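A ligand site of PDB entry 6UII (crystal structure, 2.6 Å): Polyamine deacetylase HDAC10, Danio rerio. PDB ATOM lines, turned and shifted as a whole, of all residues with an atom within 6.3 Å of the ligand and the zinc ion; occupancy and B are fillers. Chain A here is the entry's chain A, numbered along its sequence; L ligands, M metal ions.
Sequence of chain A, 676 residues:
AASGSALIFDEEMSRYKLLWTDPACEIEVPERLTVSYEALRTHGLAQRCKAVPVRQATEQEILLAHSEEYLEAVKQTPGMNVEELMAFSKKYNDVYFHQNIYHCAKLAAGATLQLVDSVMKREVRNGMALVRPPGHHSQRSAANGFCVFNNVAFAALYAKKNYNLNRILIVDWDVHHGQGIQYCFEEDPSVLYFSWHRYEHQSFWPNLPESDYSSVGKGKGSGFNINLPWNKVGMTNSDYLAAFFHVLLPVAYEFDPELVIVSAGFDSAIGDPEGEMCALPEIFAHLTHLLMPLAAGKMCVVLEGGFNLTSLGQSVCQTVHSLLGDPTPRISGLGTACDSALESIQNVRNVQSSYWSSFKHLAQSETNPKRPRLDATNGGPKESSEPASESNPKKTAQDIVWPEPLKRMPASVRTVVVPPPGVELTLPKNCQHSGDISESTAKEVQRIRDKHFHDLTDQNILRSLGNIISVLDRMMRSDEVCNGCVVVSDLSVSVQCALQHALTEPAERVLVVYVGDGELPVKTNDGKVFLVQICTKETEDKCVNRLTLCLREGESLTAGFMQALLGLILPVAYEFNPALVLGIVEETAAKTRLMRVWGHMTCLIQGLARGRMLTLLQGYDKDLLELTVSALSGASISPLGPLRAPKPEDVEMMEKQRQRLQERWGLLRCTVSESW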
ATOM      1  N   PRO A  23      15.357  -9.147  26.673  1.00  0.00           N
ATOM      2  CA  PRO A  23      16.452  -8.209  26.377  1.00  0.00           C
ATOM      3  C   PRO A  23      17.695  -8.871  25.816  1.00  0.00           C
ATOM      4  O   PRO A  23      18.526  -8.178  25.211  1.00  0.00           O
ATOM      5  CB  PRO A  23      16.720  -7.547  27.735  1.00  0.00           C
ATOM      6  CG  PRO A  23      15.458  -7.776  28.540  1.00  0.00           C
ATOM      7  CD  PRO A  23      14.956  -9.112  28.091  1.00  0.00           C
ATOM      8  N   ALA A  24      17.845 -10.184  25.986  1.00  0.00           N
ATOM      9  CA  ALA A  24      19.027 -10.855  25.460  1.00  0.00           C
ATOM     10  C   ALA A  24      19.002 -11.003  23.939  1.00  0.00           C
ATOM     11  O   ALA A  24      20.063 -10.989  23.305  1.00  0.00           O
ATOM     12  CB  ALA A  24      19.180 -12.239  26.108  1.00  0.00           C
ATOM     13  N   CYS A  25      17.821 -11.171  23.333  1.00  0.00           N
ATOM     14  CA  CYS A  25      17.737 -11.443  21.898  1.00  0.00           C
ATOM     15  C   CYS A  25      17.067 -10.351  21.092  1.00  0.00           C
ATOM     16  O   CYS A  25      16.916 -10.516  19.865  1.00  0.00           O
ATOM     17  CB  CYS A  25      17.018 -12.776  21.631  1.00  0.00           C
ATOM     18  SG  CYS A  25      17.376 -14.137  22.761  1.00  0.00           S
ATOM     19  N   ILE A  27      18.221  -7.662  19.954  1.00  0.00           N
ATOM     20  CA  ILE A  27      19.061  -7.065  18.934  1.00  0.00           C
ATOM     21  C   ILE A  27      19.082  -7.881  17.644  1.00  0.00           C
ATOM     22  O   ILE A  27      19.479  -7.344  16.598  1.00  0.00           O
ATOM     23  CB  ILE A  27      20.494  -6.851  19.469  1.00  0.00           C
ATOM     24  CG1 ILE A  27      21.188  -8.191  19.679  1.00  0.00           C
ATOM     25  CG2 ILE A  27      20.454  -6.071  20.764  1.00  0.00           C
ATOM     26  CD1 ILE A  27      22.671  -8.071  19.904  1.00  0.00           C
ATOM     27  N   GLU A  28      18.668  -9.141  17.680  1.00  0.00           N
ATOM     28  CA  GLU A  28      18.756 -10.032  16.509  1.00  0.00           C
ATOM     29  C   GLU A  28      17.425 -10.015  15.758  1.00  0.00           C
ATOM     30  O   GLU A  28      16.472 -10.693  16.150  1.00  0.00           O
ATOM     31  CB  GLU A  28      19.137 -11.441  16.942  1.00  0.00           C
ATOM     32  CG  GLU A  28      20.028 -12.164  15.942  1.00  0.00           C
ATOM     33  CD  GLU A  28      19.273 -12.597  14.704  1.00  0.00           C
ATOM     34  OE1 GLU A  28      18.274 -13.321  14.843  1.00  0.00           O
ATOM     35  OE2 GLU A  28      19.692 -12.198  13.590  1.00  0.00           O
ATOM     36  N   ASP A  94      20.429 -17.678  25.580  1.00  0.00           N
ATOM     37  CA  ASP A  94      20.392 -16.513  24.702  1.00  0.00           C
ATOM     38  C   ASP A  94      20.063 -16.905  23.253  1.00  0.00           C
ATOM     39  O   ASP A  94      20.791 -16.578  22.311  1.00  0.00           O
ATOM     40  CB  ASP A  94      21.714 -15.730  24.777  1.00  0.00           C
ATOM     41  CG  ASP A  94      21.838 -14.943  26.057  1.00  0.00           C
ATOM     42  OD1 ASP A  94      20.855 -14.851  26.824  1.00  0.00           O
ATOM     43  OD2 ASP A  94      22.933 -14.401  26.300  1.00  0.00           O
ATOM     44  N   PRO A 134      22.580 -17.093  12.679  1.00  0.00           N
ATOM     45  CA  PRO A 134      24.029 -17.320  12.690  1.00  0.00           C
ATOM     46  C   PRO A 134      24.370 -18.741  13.110  1.00  0.00           C
ATOM     47  O   PRO A 134      23.477 -19.537  13.429  1.00  0.00           O
ATOM     48  CB  PRO A 134      24.542 -16.301  13.712  1.00  0.00           C
ATOM     49  CG  PRO A 134      23.447 -15.297  13.847  1.00  0.00           C
ATOM     50  CD  PRO A 134      22.190 -16.070  13.659  1.00  0.00           C
ATOM     51  N   HIS A 136      28.121 -19.741  14.598  1.00  0.00           N
ATOM     52  CA  HIS A 136      29.377 -20.112  15.245  1.00  0.00           C
ATOM     53  C   HIS A 136      29.246 -20.440  16.725  1.00  0.00           C
ATOM     54  O   HIS A 136      30.165 -21.029  17.284  1.00  0.00           O
ATOM     55  CB  HIS A 136      30.433 -19.016  15.039  1.00  0.00           C
ATOM     56  CG  HIS A 136      30.100 -17.705  15.676  1.00  0.00           C
ATOM     57  ND1 HIS A 136      31.008 -16.667  15.745  1.00  0.00           N
ATOM     58  CD2 HIS A 136      28.964 -17.248  16.247  1.00  0.00           C
ATOM     59  CE1 HIS A 136      30.440 -15.627  16.320  1.00  0.00           C
ATOM     60  NE2 HIS A 136      29.196 -15.949  16.643  1.00  0.00           N
ATOM     61  N   HIS A 137      28.131 -20.102  17.355  1.00  0.00           N
ATOM     62  CA  HIS A 137      27.923 -20.415  18.765  1.00  0.00           C
ATOM     63  C   HIS A 137      27.267 -21.771  18.983  1.00  0.00           C
ATOM     64  O   HIS A 137      27.398 -22.329  20.081  1.00  0.00           O
ATOM     65  CB  HIS A 137      27.056 -19.342  19.422  1.00  0.00           C
ATOM     66  CG  HIS A 137      27.695 -17.993  19.481  1.00  0.00           C
ATOM     67  ND1 HIS A 137      29.003 -17.818  19.888  1.00  0.00           N
ATOM     68  CD2 HIS A 137      27.216 -16.774  19.174  1.00  0.00           C
ATOM     69  CE1 HIS A 137      29.294 -16.530  19.837  1.00  0.00           C
ATOM     70  NE2 HIS A 137      28.235 -15.874  19.414  1.00  0.00           N
ATOM     71  N   GLY A 145      23.285 -18.529  21.615  1.00  0.00           N
ATOM     72  CA  GLY A 145      23.632 -17.226  21.085  1.00  0.00           C
ATOM     73  C   GLY A 145      23.102 -16.971  19.688  1.00  0.00           C
ATOM     74  O   GLY A 145      23.891 -16.733  18.754  1.00  0.00           O
ATOM     75  N   PHE A 146      21.786 -17.046  19.527  1.00  0.00           N
ATOM     76  CA  PHE A 146      21.037 -16.815  18.286  1.00  0.00           C
ATOM     77  C   PHE A 146      21.286 -17.891  17.232  1.00  0.00           C
ATOM     78  O   PHE A 146      20.712 -17.799  16.142  1.00  0.00           O
ATOM     79  CB  PHE A 146      21.340 -15.439  17.657  1.00  0.00           C
ATOM     80  CG  PHE A 146      21.295 -14.285  18.633  1.00  0.00           C
ATOM     81  CD1 PHE A 146      20.476 -14.327  19.748  1.00  0.00           C
ATOM     82  CD2 PHE A 146      22.084 -13.161  18.433  1.00  0.00           C
ATOM     83  CE1 PHE A 146      20.443 -13.270  20.637  1.00  0.00           C
ATOM     84  CE2 PHE A 146      22.040 -12.100  19.327  1.00  0.00           C
ATOM     85  CZ  PHE A 146      21.225 -12.157  20.427  1.00  0.00           C
ATOM     86  N   CYS A 147      22.095 -18.915  17.518  1.00  0.00           N
ATOM     87  CA  CYS A 147      22.502 -19.911  16.535  1.00  0.00           C
ATOM     88  C   CYS A 147      21.742 -21.219  16.752  1.00  0.00           C
ATOM     89  O   CYS A 147      21.582 -21.658  17.895  1.00  0.00           O
ATOM     90  CB  CYS A 147      23.994 -20.194  16.627  1.00  0.00           C
ATOM     91  SG  CYS A 147      25.057 -18.744  16.453  1.00  0.00           S
ATOM     92  N   ASP A 174      34.048 -12.152  13.955  1.00  0.00           N
ATOM     93  CA  ASP A 174      32.955 -11.703  14.817  1.00  0.00           C
ATOM     94  C   ASP A 174      33.517 -11.315  16.194  1.00  0.00           C
ATOM     95  O   ASP A 174      34.562 -11.817  16.629  1.00  0.00           O
ATOM     96  CB  ASP A 174      31.914 -12.823  14.936  1.00  0.00           C
ATOM     97  CG  ASP A 174      30.641 -12.370  15.611  1.00  0.00           C
ATOM     98  OD1 ASP A 174      29.628 -12.159  14.913  1.00  0.00           O
ATOM     99  OD2 ASP A 174      30.631 -12.237  16.839  1.00  0.00           O
ATOM    100  N   VAL A 175      32.813 -10.395  16.878  1.00  0.00           N
ATOM    101  CA  VAL A 175      33.282  -9.933  18.192  1.00  0.00           C
ATOM    102  C   VAL A 175      33.027 -10.949  19.296  1.00  0.00           C
ATOM    103  O   VAL A 175      33.617 -10.826  20.377  1.00  0.00           O
ATOM    104  CB  VAL A 175      32.623  -8.588  18.560  1.00  0.00           C
ATOM    105  CG1 VAL A 175      31.256  -8.798  19.237  1.00  0.00           C
ATOM    106  CG2 VAL A 175      33.546  -7.749  19.448  1.00  0.00           C
ATOM    107  N   HIS A 176      32.177 -11.944  19.066  1.00  0.00           N
ATOM    108  CA  HIS A 176      31.959 -13.013  20.023  1.00  0.00           C
ATOM    109  C   HIS A 176      32.817 -14.220  19.656  1.00  0.00           C
ATOM    110  O   HIS A 176      33.250 -14.391  18.511  1.00  0.00           O
ATOM    111  CB  HIS A 176      30.495 -13.437  20.065  1.00  0.00           C
ATOM    112  CG  HIS A 176      29.558 -12.334  20.401  1.00  0.00           C
ATOM    113  ND1 HIS A 176      29.192 -11.354  19.496  1.00  0.00           N
ATOM    114  CD2 HIS A 176      28.896 -12.049  21.550  1.00  0.00           C
ATOM    115  CE1 HIS A 176      28.348 -10.517  20.071  1.00  0.00           C
ATOM    116  NE2 HIS A 176      28.156 -10.913  21.322  1.00  0.00           N
ATOM    117  N   HIS A 177      33.048 -15.069  20.655  1.00  0.00           N
ATOM    118  CA  HIS A 177      33.868 -16.266  20.472  1.00  0.00           C
ATOM    119  C   HIS A 177      33.024 -17.371  19.852  1.00  0.00           C
ATOM    120  O   HIS A 177      31.941 -17.682  20.362  1.00  0.00           O
ATOM    121  CB  HIS A 177      34.480 -16.707  21.795  1.00  0.00           C
ATOM    122  CG  HIS A 177      35.345 -17.933  21.674  1.00  0.00           C
ATOM    123  ND1 HIS A 177      35.143 -19.063  22.431  1.00  0.00           N
ATOM    124  CD2 HIS A 177      36.405 -18.200  20.873  1.00  0.00           C
ATOM    125  CE1 HIS A 177      36.039 -19.973  22.106  1.00  0.00           C
ATOM    126  NE2 HIS A 177      36.819 -19.471  21.160  1.00  0.00           N
ATOM    127  N   PHE A 204      32.755 -10.994  29.743  1.00  0.00           N
ATOM    128  CA  PHE A 204      31.840 -10.819  28.623  1.00  0.00           C
ATOM    129  C   PHE A 204      31.376 -12.158  28.066  1.00  0.00           C
ATOM    130  O   PHE A 204      32.126 -13.144  28.034  1.00  0.00           O
ATOM    131  CB  PHE A 204      32.482 -10.002  27.505  1.00  0.00           C
ATOM    132  CG  PHE A 204      31.515  -9.580  26.439  1.00  0.00           C
ATOM    133  CD1 PHE A 204      30.528  -8.638  26.707  1.00  0.00           C
ATOM    134  CD2 PHE A 204      31.563 -10.155  25.171  1.00  0.00           C
ATOM    135  CE1 PHE A 204      29.621  -8.274  25.730  1.00  0.00           C
ATOM    136  CE2 PHE A 204      30.653  -9.789  24.203  1.00  0.00           C
ATOM    137  CZ  PHE A 204      29.681  -8.847  24.487  1.00  0.00           C
ATOM    138  N   TRP A 205      30.114 -12.175  27.614  1.00  0.00           N
ATOM    139  CA  TRP A 205      29.456 -13.376  27.114  1.00  0.00           C
ATOM    140  C   TRP A 205      30.285 -14.006  25.989  1.00  0.00           C
ATOM    141  O   TRP A 205      30.823 -13.293  25.134  1.00  0.00           O
ATOM    142  CB  TRP A 205      28.052 -13.018  26.614  1.00  0.00           C
ATOM    143  CG  TRP A 205      27.183 -14.198  26.337  1.00  0.00           C
ATOM    144  CD1 TRP A 205      26.271 -14.751  27.189  1.00  0.00           C
ATOM    145  CD2 TRP A 205      27.140 -14.969  25.129  1.00  0.00           C
ATOM    146  NE1 TRP A 205      25.679 -15.834  26.586  1.00  0.00           N
ATOM    147  CE2 TRP A 205      26.188 -15.987  25.330  1.00  0.00           C
ATOM    148  CE3 TRP A 205      27.821 -14.893  23.913  1.00  0.00           C
ATOM    149  CZ2 TRP A 205      25.896 -16.930  24.338  1.00  0.00           C
ATOM    150  CZ3 TRP A 205      27.535 -15.834  22.935  1.00  0.00           C
ATOM    151  CH2 TRP A 205      26.575 -16.835  23.159  1.00  0.00           C
ATOM    152  N   GLY A 265      31.272 -11.768  11.249  1.00  0.00           N
ATOM    153  CA  GLY A 265      30.369 -10.967  12.061  1.00  0.00           C
ATOM    154  C   GLY A 265      30.857  -9.533  12.042  1.00  0.00           C
ATOM    155  O   GLY A 265      32.061  -9.284  12.144  1.00  0.00           O
ATOM    156  N   ASP A 267      29.506  -7.176  14.164  1.00  0.00           N
ATOM    157  CA  ASP A 267      29.413  -6.616  15.499  1.00  0.00           C
ATOM    158  C   ASP A 267      30.779  -6.240  16.066  1.00  0.00           C
ATOM    159  O   ASP A 267      30.838  -5.734  17.198  1.00  0.00           O
ATOM    160  CB  ASP A 267      28.711  -7.592  16.453  1.00  0.00           C
ATOM    161  CG  ASP A 267      29.263  -9.003  16.369  1.00  0.00           C
ATOM    162  OD1 ASP A 267      30.340  -9.209  15.769  1.00  0.00           O
ATOM    163  OD2 ASP A 267      28.619  -9.909  16.905  1.00  0.00           O
ATOM    164  N   GLU A 274      26.870  -4.259  20.820  1.00  0.00           N
ATOM    165  CA  GLU A 274      27.283  -5.485  21.487  1.00  0.00           C
ATOM    166  C   GLU A 274      28.791  -5.626  21.617  1.00  0.00           C
ATOM    167  O   GLU A 274      29.258  -6.229  22.573  1.00  0.00           O
ATOM    168  CB  GLU A 274      26.718  -6.694  20.733  1.00  0.00           C
ATOM    169  CG  GLU A 274      26.871  -8.015  21.427  1.00  0.00           C
ATOM    170  CD  GLU A 274      25.894  -8.234  22.559  1.00  0.00           C
ATOM    171  OE1 GLU A 274      26.142  -9.139  23.380  1.00  0.00           O
ATOM    172  OE2 GLU A 274      24.882  -7.486  22.644  1.00  0.00           O
ATOM    173  N   GLU A 304      27.607 -13.712  10.268  1.00  0.00           N
ATOM    174  CA  GLU A 304      27.305 -14.129  11.628  1.00  0.00           C
ATOM    175  C   GLU A 304      26.536 -12.985  12.290  1.00  0.00           C
ATOM    176  O   GLU A 304      25.355 -12.780  11.978  1.00  0.00           O
ATOM    177  CB  GLU A 304      28.575 -14.498  12.393  1.00  0.00           C
ATOM    178  CG  GLU A 304      29.388 -15.624  11.766  1.00  0.00           C
ATOM    179  CD  GLU A 304      28.853 -17.019  12.091  1.00  0.00           C
ATOM    180  OE1 GLU A 304      29.482 -17.998  11.623  1.00  0.00           O
ATOM    181  OE2 GLU A 304      27.830 -17.142  12.800  1.00  0.00           O
ATOM    182  N   GLY A 305      27.156 -12.242  13.199  1.00  0.00           N
ATOM    183  CA  GLY A 305      26.513 -11.130  13.866  1.00  0.00           C
ATOM    184  C   GLY A 305      26.790  -9.796  13.207  1.00  0.00           C
ATOM    185  O   GLY A 305      27.398  -9.701  12.135  1.00  0.00           O
ATOM    186  N   GLY A 306      26.352  -8.732  13.894  1.00  0.00           N
ATOM    187  CA  GLY A 306      26.322  -7.370  13.383  1.00  0.00           C
ATOM    188  C   GLY A 306      24.926  -6.806  13.565  1.00  0.00           C
ATOM    189  O   GLY A 306      24.024  -7.159  12.795  1.00  0.00           O
ATOM    190  N   PHE A 307      24.718  -5.952  14.574  1.00  0.00           N
ATOM    191  CA  PHE A 307      23.370  -5.635  15.027  1.00  0.00           C
ATOM    192  C   PHE A 307      23.027  -4.157  14.993  1.00  0.00           C
ATOM    193  O   PHE A 307      21.921  -3.782  15.424  1.00  0.00           O
ATOM    194  CB  PHE A 307      23.163  -6.190  16.449  1.00  0.00           C
ATOM    195  CG  PHE A 307      23.559  -7.618  16.578  1.00  0.00           C
ATOM    196  CD1 PHE A 307      22.658  -8.624  16.286  1.00  0.00           C
ATOM    197  CD2 PHE A 307      24.856  -7.966  16.951  1.00  0.00           C
ATOM    198  CE1 PHE A 307      23.030  -9.948  16.381  1.00  0.00           C
ATOM    199  CE2 PHE A 307      25.224  -9.287  17.055  1.00  0.00           C
ATOM    200  CZ  PHE A 307      24.313 -10.279  16.766  1.00  0.00           C
HETATM  201  C1  LIG L   1      22.524 -10.105  24.804  1.00  0.00           C
HETATM  202  C2  LIG L   1      23.864 -10.812  24.625  1.00  0.00           C
HETATM  203  C3  LIG L   1      23.640 -12.250  24.188  1.00  0.00           C
HETATM  204  C4  LIG L   1      24.283 -13.328  22.131  1.00  0.00           C
HETATM  205  C5  LIG L   1      25.453 -13.588  21.214  1.00  0.00           C
HETATM  206  C6  LIG L   1      25.249 -12.802  19.965  1.00  0.00           C
HETATM  207  C7  LIG L   1      26.389 -13.020  19.056  1.00  0.00           C
HETATM  208  C8  LIG L   1      25.882 -13.451  17.738  1.00  0.00           C
HETATM  209  N1  LIG L   1      22.602  -8.689  25.166  1.00  0.00           N
HETATM  210  N2  LIG L   1      24.760 -12.669  23.349  1.00  0.00           N
HETATM  211  S1  LIG L   1      27.336 -13.503  16.709  1.00  0.00           S
HETATM  212 ZN    ZN M   1      28.775 -11.841  17.386  1.00  0.00          ZN
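NE2 of His 136 sits close to S1 of the ligand, 3.1 Å away.
N1 of the ligand lies within salt-bridge range of OE2 of Glu 274.
S1 of the ligand sits close to N of Gly 305, at 3.7 Å.
OD2 of Asp 94 lies within salt-bridge range of N2 of the ligand, at 3.9 Å.
A ring nitrogen (NE2) of His 137 sits close to a sulfur (S1) of the ligand, at 3.7 Å.
N of Gly 145 lies close to O of Asp 94 (3.2 Å).
The side-chain sulfur (SG) of Cys 147 lies within hydrogen-bond range of the backbone carbonyl oxygen (O) of Gly 145 (3.3 Å).
The side-chain carboxylate (OD1) of Asp 174 sits at hydrogen-bond distance from the backbone NH (N) of Gly 305 (3.0 Å).
N of His 137 is in hydrogen-bond range of SG of Cys 147, 3.5 Å away.
The backbone carbonyl oxygen of His 177 lies close to a ring nitrogen (ND1) of His 137.
The backbone carbonyl oxygen (O) of Asp 94 lies within hydrogen-bond range of the backbone NH (N) of Phe 146, at 3.0 Å.
A ring nitrogen (NE2) of His 176 sits close to the side-chain carboxylate (OE1) of Glu 274 (3.4 Å).
The side-chain carboxylate of Glu 304 is in hydrogen-bond range of the backbone NH of His 136.
Merely in contact with the ligand: Ala 24, Gly 145, Phe 146, Trp 205 and Phe 307.
Hydrophobic or aromatic side chains that line the ligand: His 136, His 137, Phe 146, His 176, Trp 205 and Phe 307.
Of the 25 residues printed, 13 come within 4 Å of the ligand.
Three residues have an atom within 4 Å of the zinc ion: Asp 174, His 176 and Asp 267.
The nearest printed residue that does not touch the zinc ion is His 136 (4.2 Å).
The zinc ion is bound by OD2 of Asp 174 (2.0 Å), OD2 of Asp 267 (2.0 Å), ND1 of His 176 (2.2 Å) and S1 of the ligand (2.3 Å).
The zinc ion has four donor atoms within binding distance.
Slightly farther from the zinc ion lies OD1 of Asp 174 (2.6 Å).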
